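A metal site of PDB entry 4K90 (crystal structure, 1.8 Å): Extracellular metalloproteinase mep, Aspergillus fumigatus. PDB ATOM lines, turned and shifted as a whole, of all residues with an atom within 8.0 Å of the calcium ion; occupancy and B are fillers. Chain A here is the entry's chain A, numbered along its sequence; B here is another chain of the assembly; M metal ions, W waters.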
ATOM      1  N   ALA A 117      -5.557  11.109 -37.137  1.00  0.00           N
ATOM      2  CA  ALA A 117      -4.808  11.386 -35.888  1.00  0.00           C
ATOM      3  C   ALA A 117      -5.495  10.867 -34.626  1.00  0.00           C
ATOM      4  O   ALA A 117      -5.062  11.167 -33.511  1.00  0.00           O
ATOM      5  CB  ALA A 117      -4.504  12.910 -35.764  1.00  0.00           C
ATOM      6  N   GLY A 118      -6.554  10.068 -34.787  1.00  0.00           N
ATOM      7  CA  GLY A 118      -7.212   9.403 -33.666  1.00  0.00           C
ATOM      8  C   GLY A 118      -8.279  10.230 -32.959  1.00  0.00           C
ATOM      9  O   GLY A 118      -8.486  10.082 -31.749  1.00  0.00           O
ATOM     10  N   THR A 152     -10.406   7.662 -21.922  1.00  0.00           N
ATOM     11  CA  THR A 152      -9.824   7.623 -23.265  1.00  0.00           C
ATOM     12  C   THR A 152      -9.307   6.225 -23.614  1.00  0.00           C
ATOM     13  O   THR A 152      -8.097   5.970 -23.510  1.00  0.00           O
ATOM     14  CB  THR A 152      -8.712   8.685 -23.474  1.00  0.00           C
ATOM     15  OG1 THR A 152      -9.158   9.960 -23.021  1.00  0.00           O
ATOM     16  CG2 THR A 152      -8.367   8.795 -24.978  1.00  0.00           C
ATOM     17  N   PRO A 153     -10.214   5.325 -24.053  1.00  0.00           N
ATOM     18  CA  PRO A 153      -9.747   4.066 -24.607  1.00  0.00           C
ATOM     19  C   PRO A 153      -9.082   4.343 -25.978  1.00  0.00           C
ATOM     20  O   PRO A 153      -9.135   5.474 -26.462  1.00  0.00           O
ATOM     21  CB  PRO A 153     -11.042   3.272 -24.784  1.00  0.00           C
ATOM     22  CG  PRO A 153     -12.099   4.321 -25.038  1.00  0.00           C
ATOM     23  CD  PRO A 153     -11.693   5.447 -24.110  1.00  0.00           C
ATOM     24  N   PRO A 154      -8.452   3.329 -26.590  1.00  0.00           N
ATOM     25  CA  PRO A 154      -7.795   3.560 -27.870  1.00  0.00           C
ATOM     26  C   PRO A 154      -8.788   3.929 -28.976  1.00  0.00           C
ATOM     27  O   PRO A 154      -9.997   3.781 -28.801  1.00  0.00           O
ATOM     28  CB  PRO A 154      -7.118   2.217 -28.191  1.00  0.00           C
ATOM     29  CG  PRO A 154      -7.028   1.520 -26.850  1.00  0.00           C
ATOM     30  CD  PRO A 154      -8.280   1.935 -26.140  1.00  0.00           C
ATOM     31  N   ASP A 155      -8.245   4.423 -30.087  1.00  0.00           N
ATOM     32  CA  ASP A 155      -9.030   4.817 -31.251  1.00  0.00           C
ATOM     33  C   ASP A 155     -10.035   3.739 -31.625  1.00  0.00           C
ATOM     34  O   ASP A 155      -9.709   2.537 -31.589  1.00  0.00           O
ATOM     35  CB  ASP A 155      -8.123   5.089 -32.445  1.00  0.00           C
ATOM     36  CG  ASP A 155      -8.756   6.040 -33.459  1.00  0.00           C
ATOM     37  OD1 ASP A 155      -9.770   6.715 -33.109  1.00  0.00           O
ATOM     38  OD2 ASP A 155      -8.238   6.136 -34.592  1.00  0.00           O
ATOM     39  N   GLY A 189      -8.666  13.361 -23.668  1.00  0.00           N
ATOM     40  CA  GLY A 189      -8.855  12.570 -24.889  1.00  0.00           C
ATOM     41  C   GLY A 189      -7.837  12.916 -25.953  1.00  0.00           C
ATOM     42  O   GLY A 189      -7.224  12.024 -26.552  1.00  0.00           O
ATOM     43  N   LEU A 190      -7.637  14.210 -26.180  1.00  0.00           N
ATOM     44  CA  LEU A 190      -6.672  14.678 -27.154  1.00  0.00           C
ATOM     45  C   LEU A 190      -5.268  14.154 -26.861  1.00  0.00           C
ATOM     46  O   LEU A 190      -4.594  13.583 -27.740  1.00  0.00           O
ATOM     47  CB  LEU A 190      -6.634  16.214 -27.164  1.00  0.00           C
ATOM     48  CG  LEU A 190      -5.527  16.852 -28.003  1.00  0.00           C
ATOM     49  CD1 LEU A 190      -5.778  16.685 -29.526  1.00  0.00           C
ATOM     50  CD2 LEU A 190      -5.371  18.306 -27.612  1.00  0.00           C
ATOM     51  N   SER A 191      -4.813  14.373 -25.634  1.00  0.00           N
ATOM     52  CA  SER A 191      -3.421  14.085 -25.295  1.00  0.00           C
ATOM     53  C   SER A 191      -3.193  12.585 -25.255  1.00  0.00           C
ATOM     54  O   SER A 191      -2.174  12.101 -25.753  1.00  0.00           O
ATOM     55  CB  SER A 191      -3.028  14.786 -23.993  1.00  0.00           C
ATOM     56  OG  SER A 191      -3.806  14.303 -22.907  1.00  0.00           O
ATOM     57  N   ASN A 192      -4.144  11.815 -24.715  1.00  0.00           N
ATOM     58  CA  ASN A 192      -4.001  10.363 -24.685  1.00  0.00           C
ATOM     59  C   ASN A 192      -4.052   9.719 -26.068  1.00  0.00           C
ATOM     60  O   ASN A 192      -3.314   8.762 -26.342  1.00  0.00           O
ATOM     61  CB  ASN A 192      -5.008   9.722 -23.744  1.00  0.00           C
ATOM     62  CG  ASN A 192      -4.513   9.734 -22.322  1.00  0.00           C
ATOM     63  OD1 ASN A 192      -3.543   9.045 -22.005  1.00  0.00           O
ATOM     64  ND2 ASN A 192      -5.148  10.552 -21.467  1.00  0.00           N
ATOM     65  N   ARG A 193      -4.909  10.248 -26.948  1.00  0.00           N
ATOM     66  CA  ARG A 193      -4.957   9.742 -28.332  1.00  0.00           C
ATOM     67  C   ARG A 193      -3.679  10.066 -29.086  1.00  0.00           C
ATOM     68  O   ARG A 193      -3.058   9.168 -29.666  1.00  0.00           O
ATOM     69  CB  ARG A 193      -6.195  10.257 -29.086  1.00  0.00           C
ATOM     70  CG  ARG A 193      -7.511   9.609 -28.618  1.00  0.00           C
ATOM     71  CD  ARG A 193      -7.636   8.161 -29.081  1.00  0.00           C
ATOM     72  NE  ARG A 193      -8.815   7.448 -28.572  1.00  0.00           N
ATOM     73  CZ  ARG A 193     -10.030   7.518 -29.114  1.00  0.00           C
ATOM     74  NH1 ARG A 193     -10.242   8.339 -30.163  1.00  0.00           N
ATOM     75  NH2 ARG A 193     -11.041   6.789 -28.628  1.00  0.00           N
ATOM     76  N   LEU A 194      -3.256  11.334 -29.090  1.00  0.00           N
ATOM     77  CA  LEU A 194      -2.063  11.705 -29.854  1.00  0.00           C
ATOM     78  C   LEU A 194      -0.790  11.045 -29.316  1.00  0.00           C
ATOM     79  O   LEU A 194       0.058  10.558 -30.099  1.00  0.00           O
ATOM     80  CB  LEU A 194      -1.891  13.232 -29.879  1.00  0.00           C
ATOM     81  CG  LEU A 194      -2.881  13.971 -30.784  1.00  0.00           C
ATOM     82  CD1 LEU A 194      -2.612  15.456 -30.661  1.00  0.00           C
ATOM     83  CD2 LEU A 194      -2.715  13.525 -32.264  1.00  0.00           C
ATOM     84  N   THR A 195      -0.637  11.006 -27.994  1.00  0.00           N
ATOM     85  CA  THR A 195       0.592  10.445 -27.407  1.00  0.00           C
ATOM     86  C   THR A 195       0.690   8.935 -27.647  1.00  0.00           C
ATOM     87  O   THR A 195      -0.242   8.176 -27.310  1.00  0.00           O
ATOM     88  CB  THR A 195       0.717  10.759 -25.906  1.00  0.00           C
ATOM     89  OG1 THR A 195       0.586  12.177 -25.705  1.00  0.00           O
ATOM     90  CG2 THR A 195       2.099  10.304 -25.390  1.00  0.00           C
ATOM     91  N   GLY A 196       1.810   8.494 -28.232  1.00  0.00           N
ATOM     92  CA  GLY A 196       2.023   7.051 -28.543  1.00  0.00           C
ATOM     93  C   GLY A 196       1.191   6.534 -29.710  1.00  0.00           C
ATOM     94  O   GLY A 196       1.191   5.331 -30.007  1.00  0.00           O
ATOM     95  N   GLY A 197       0.501   7.447 -30.391  1.00  0.00           N
ATOM     96  CA  GLY A 197      -0.334   7.085 -31.545  1.00  0.00           C
ATOM     97  C   GLY A 197      -1.734   6.682 -31.121  1.00  0.00           C
ATOM     98  O   GLY A 197      -1.960   6.245 -29.979  1.00  0.00           O
ATOM     99  N   PRO A 198      -2.716   6.832 -32.039  1.00  0.00           N
ATOM    100  CA  PRO A 198      -4.115   6.533 -31.725  1.00  0.00           C
ATOM    101  C   PRO A 198      -4.376   5.149 -31.103  1.00  0.00           C
ATOM    102  O   PRO A 198      -5.296   5.031 -30.276  1.00  0.00           O
ATOM    103  CB  PRO A 198      -4.801   6.670 -33.089  1.00  0.00           C
ATOM    104  CG  PRO A 198      -3.976   7.789 -33.778  1.00  0.00           C
ATOM    105  CD  PRO A 198      -2.548   7.373 -33.397  1.00  0.00           C
ATOM    106  N   ALA A 199      -3.584   4.144 -31.475  1.00  0.00           N
ATOM    107  CA  ALA A 199      -3.836   2.776 -31.014  1.00  0.00           C
ATOM    108  C   ALA A 199      -3.428   2.541 -29.553  1.00  0.00           C
ATOM    109  O   ALA A 199      -3.804   1.522 -28.959  1.00  0.00           O
ATOM    110  CB  ALA A 199      -3.154   1.743 -31.938  1.00  0.00           C
ATOM    111  N   ASN A 200      -2.672   3.462 -28.965  1.00  0.00           N
ATOM    112  CA  ASN A 200      -2.104   3.218 -27.632  1.00  0.00           C
ATOM    113  C   ASN A 200      -2.544   4.264 -26.617  1.00  0.00           C
ATOM    114  O   ASN A 200      -2.114   5.415 -26.679  1.00  0.00           O
ATOM    115  CB  ASN A 200      -0.571   3.134 -27.698  1.00  0.00           C
ATOM    116  CG  ASN A 200       0.033   2.525 -26.429  1.00  0.00           C
ATOM    117  OD1 ASN A 200      -0.671   2.277 -25.452  1.00  0.00           O
ATOM    118  ND2 ASN A 200       1.332   2.284 -26.455  1.00  0.00           N
ATOM    119  N   SER A 201      -3.391   3.845 -25.690  1.00  0.00           N
ATOM    120  CA  SER A 201      -3.916   4.731 -24.635  1.00  0.00           C
ATOM    121  C   SER A 201      -3.219   4.519 -23.288  1.00  0.00           C
ATOM    122  O   SER A 201      -3.684   4.999 -22.255  1.00  0.00           O
ATOM    123  CB  SER A 201      -5.426   4.572 -24.485  1.00  0.00           C
ATOM    124  OG  SER A 201      -6.083   5.322 -25.492  1.00  0.00           O
ATOM    125  N   ASN A 202      -2.086   3.819 -23.308  1.00  0.00           N
ATOM    126  CA  ASN A 202      -1.307   3.570 -22.078  1.00  0.00           C
ATOM    127  C   ASN A 202      -0.269   4.658 -21.822  1.00  0.00           C
ATOM    128  O   ASN A 202       0.512   4.564 -20.851  1.00  0.00           O
ATOM    129  CB  ASN A 202      -0.549   2.232 -22.181  1.00  0.00           C
ATOM    130  CG  ASN A 202      -1.460   1.021 -22.079  1.00  0.00           C
ATOM    131  OD1 ASN A 202      -2.671   1.121 -22.244  1.00  0.00           O
ATOM    132  ND2 ASN A 202      -0.865  -0.134 -21.807  1.00  0.00           N
ATOM    133  N   CYS A 203      -0.266   5.707 -22.639  1.00  0.00           N
ATOM    134  CA  CYS A 203       0.943   6.536 -22.823  1.00  0.00           C
ATOM    135  C   CYS A 203       1.037   7.836 -22.021  1.00  0.00           C
ATOM    136  O   CYS A 203       2.013   8.578 -22.165  1.00  0.00           O
ATOM    137  CB  CYS A 203       1.165   6.822 -24.317  1.00  0.00           C
ATOM    138  SG  CYS A 203       1.556   5.281 -25.199  1.00  0.00           S
ATOM    139  N   LEU A 204       0.025   8.113 -21.204  1.00  0.00           N
ATOM    140  CA  LEU A 204       0.107   9.223 -20.241  1.00  0.00           C
ATOM    141  C   LEU A 204      -0.342   8.728 -18.867  1.00  0.00           C
ATOM    142  O   LEU A 204      -1.220   9.320 -18.217  1.00  0.00           O
ATOM    143  CB  LEU A 204      -0.667  10.468 -20.731  1.00  0.00           C
ATOM    144  CG  LEU A 204      -0.155  11.146 -21.991  1.00  0.00           C
ATOM    145  CD1 LEU A 204      -1.124  12.268 -22.408  1.00  0.00           C
ATOM    146  CD2 LEU A 204       1.294  11.694 -21.863  1.00  0.00           C
ATOM    147  N   MET A 326       2.785  16.539 -28.929  1.00  0.00           N
ATOM    148  CA  MET A 326       2.161  15.295 -28.441  1.00  0.00           C
ATOM    149  C   MET A 326       2.338  14.145 -29.438  1.00  0.00           C
ATOM    150  O   MET A 326       2.561  13.010 -29.029  1.00  0.00           O
ATOM    151  CB  MET A 326       0.668  15.494 -28.186  1.00  0.00           C
ATOM    152  CG  MET A 326       0.341  16.474 -27.078  1.00  0.00           C
ATOM    153  SD  MET A 326      -1.445  16.771 -27.040  1.00  0.00           S
ATOM    154  CE  MET A 326      -1.508  17.828 -25.590  1.00  0.00           C
ATOM    155  N   CYS A 331       5.921   7.302 -25.873  1.00  0.00           N
ATOM    156  CA  CYS A 331       4.910   6.869 -24.945  1.00  0.00           C
ATOM    157  C   CYS A 331       5.465   7.053 -23.529  1.00  0.00           C
ATOM    158  O   CYS A 331       6.637   6.735 -23.270  1.00  0.00           O
ATOM    159  CB  CYS A 331       4.592   5.397 -25.240  1.00  0.00           C
ATOM    160  SG  CYS A 331       3.304   4.681 -24.259  1.00  0.00           S
ATOM    161  N   ASP B  59      -1.768   2.328 -37.249  1.00  0.00           N
ATOM    162  CA  ASP B  59      -2.320   3.645 -36.955  1.00  0.00           C
ATOM    163  C   ASP B  59      -1.402   4.762 -37.467  1.00  0.00           C
ATOM    164  O   ASP B  59      -1.513   5.909 -37.041  1.00  0.00           O
ATOM    165  CB  ASP B  59      -2.593   3.800 -35.429  1.00  0.00           C
ATOM    166  CG  ASP B  59      -1.301   3.850 -34.586  1.00  0.00           C
ATOM    167  OD1 ASP B  59      -0.202   3.688 -35.145  1.00  0.00           O
ATOM    168  OD2 ASP B  59      -1.407   4.093 -33.365  1.00  0.00           O
ATOM    169  N   HIS B  71       4.305   3.911 -35.456  1.00  0.00           N
ATOM    170  CA  HIS B  71       4.469   3.242 -34.174  1.00  0.00           C
ATOM    171  C   HIS B  71       4.715   1.758 -34.344  1.00  0.00           C
ATOM    172  O   HIS B  71       4.125   1.109 -35.216  1.00  0.00           O
ATOM    173  CB  HIS B  71       3.273   3.529 -33.263  1.00  0.00           C
ATOM    174  CG  HIS B  71       3.041   4.995 -33.094  1.00  0.00           C
ATOM    175  ND1 HIS B  71       3.710   5.747 -32.156  1.00  0.00           N
ATOM    176  CD2 HIS B  71       2.277   5.864 -33.802  1.00  0.00           C
ATOM    177  CE1 HIS B  71       3.344   7.013 -32.266  1.00  0.00           C
ATOM    178  NE2 HIS B  71       2.490   7.114 -33.264  1.00  0.00           N
HETATM  179 CA    CA M   1      -2.424   7.289 -27.897  1.00  0.00          CA
HETATM  180  O   HOH W   1      -4.778   6.431 -27.900  1.00  0.00           O
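SG of Cys 203 sits at hydrogen-bond distance from ND2 of Asn 200, 3.3 Å away.
The side-chain amide oxygen (OD1) of Asn 200 lies within hydrogen-bond range of the backbone NH (N) of Asn 202 (3.0 Å).
The backbone carbonyl oxygen of Ser 191 sits at hydrogen-bond distance from the side-chain hydroxyl of Thr 195 (2.8 Å).
The guanidinium group of Arg 193 is in hydrogen-bond range of the backbone carbonyl oxygen of Pro 154 (3.2 Å).
The side-chain carboxylate (OD1) of Asp 155 sits close to the guanidinium group (NH1) of Arg 193, 3.4 Å away.
The guanidinium group (NE) of Arg 193 sits at hydrogen-bond distance from the backbone carbonyl oxygen (O) of Pro 153 (2.9 Å).
NH1 of Arg 193 sits at hydrogen-bond distance from O of Gly 118, 2.9 Å away.
The side-chain sulfur (SG) of Cys 203 is disulfide-bonded to the side-chain sulfur (SG) of Cys 331.
Five residues have an atom within 4 Å of the calcium ion: Asn 192, Arg 193, Thr 195, Gly 197 and Asn 200.
The nearest printed residue that does not touch the calcium ion is Gly 196 (4.1 Å).
The calcium ion is bound by O of Asn 200 (2.3 Å), O of Asn 192 (2.3 Å), O of Gly 197 (2.4 Å), O of Thr 195 (2.4 Å), water W1 (2.5 Å) and O of Arg 193 (2.7 Å).
Water W1 lies within hydrogen-bond range of O of Pro 198 (2.8 Å) and OG of Ser 201 (3.0 Å).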
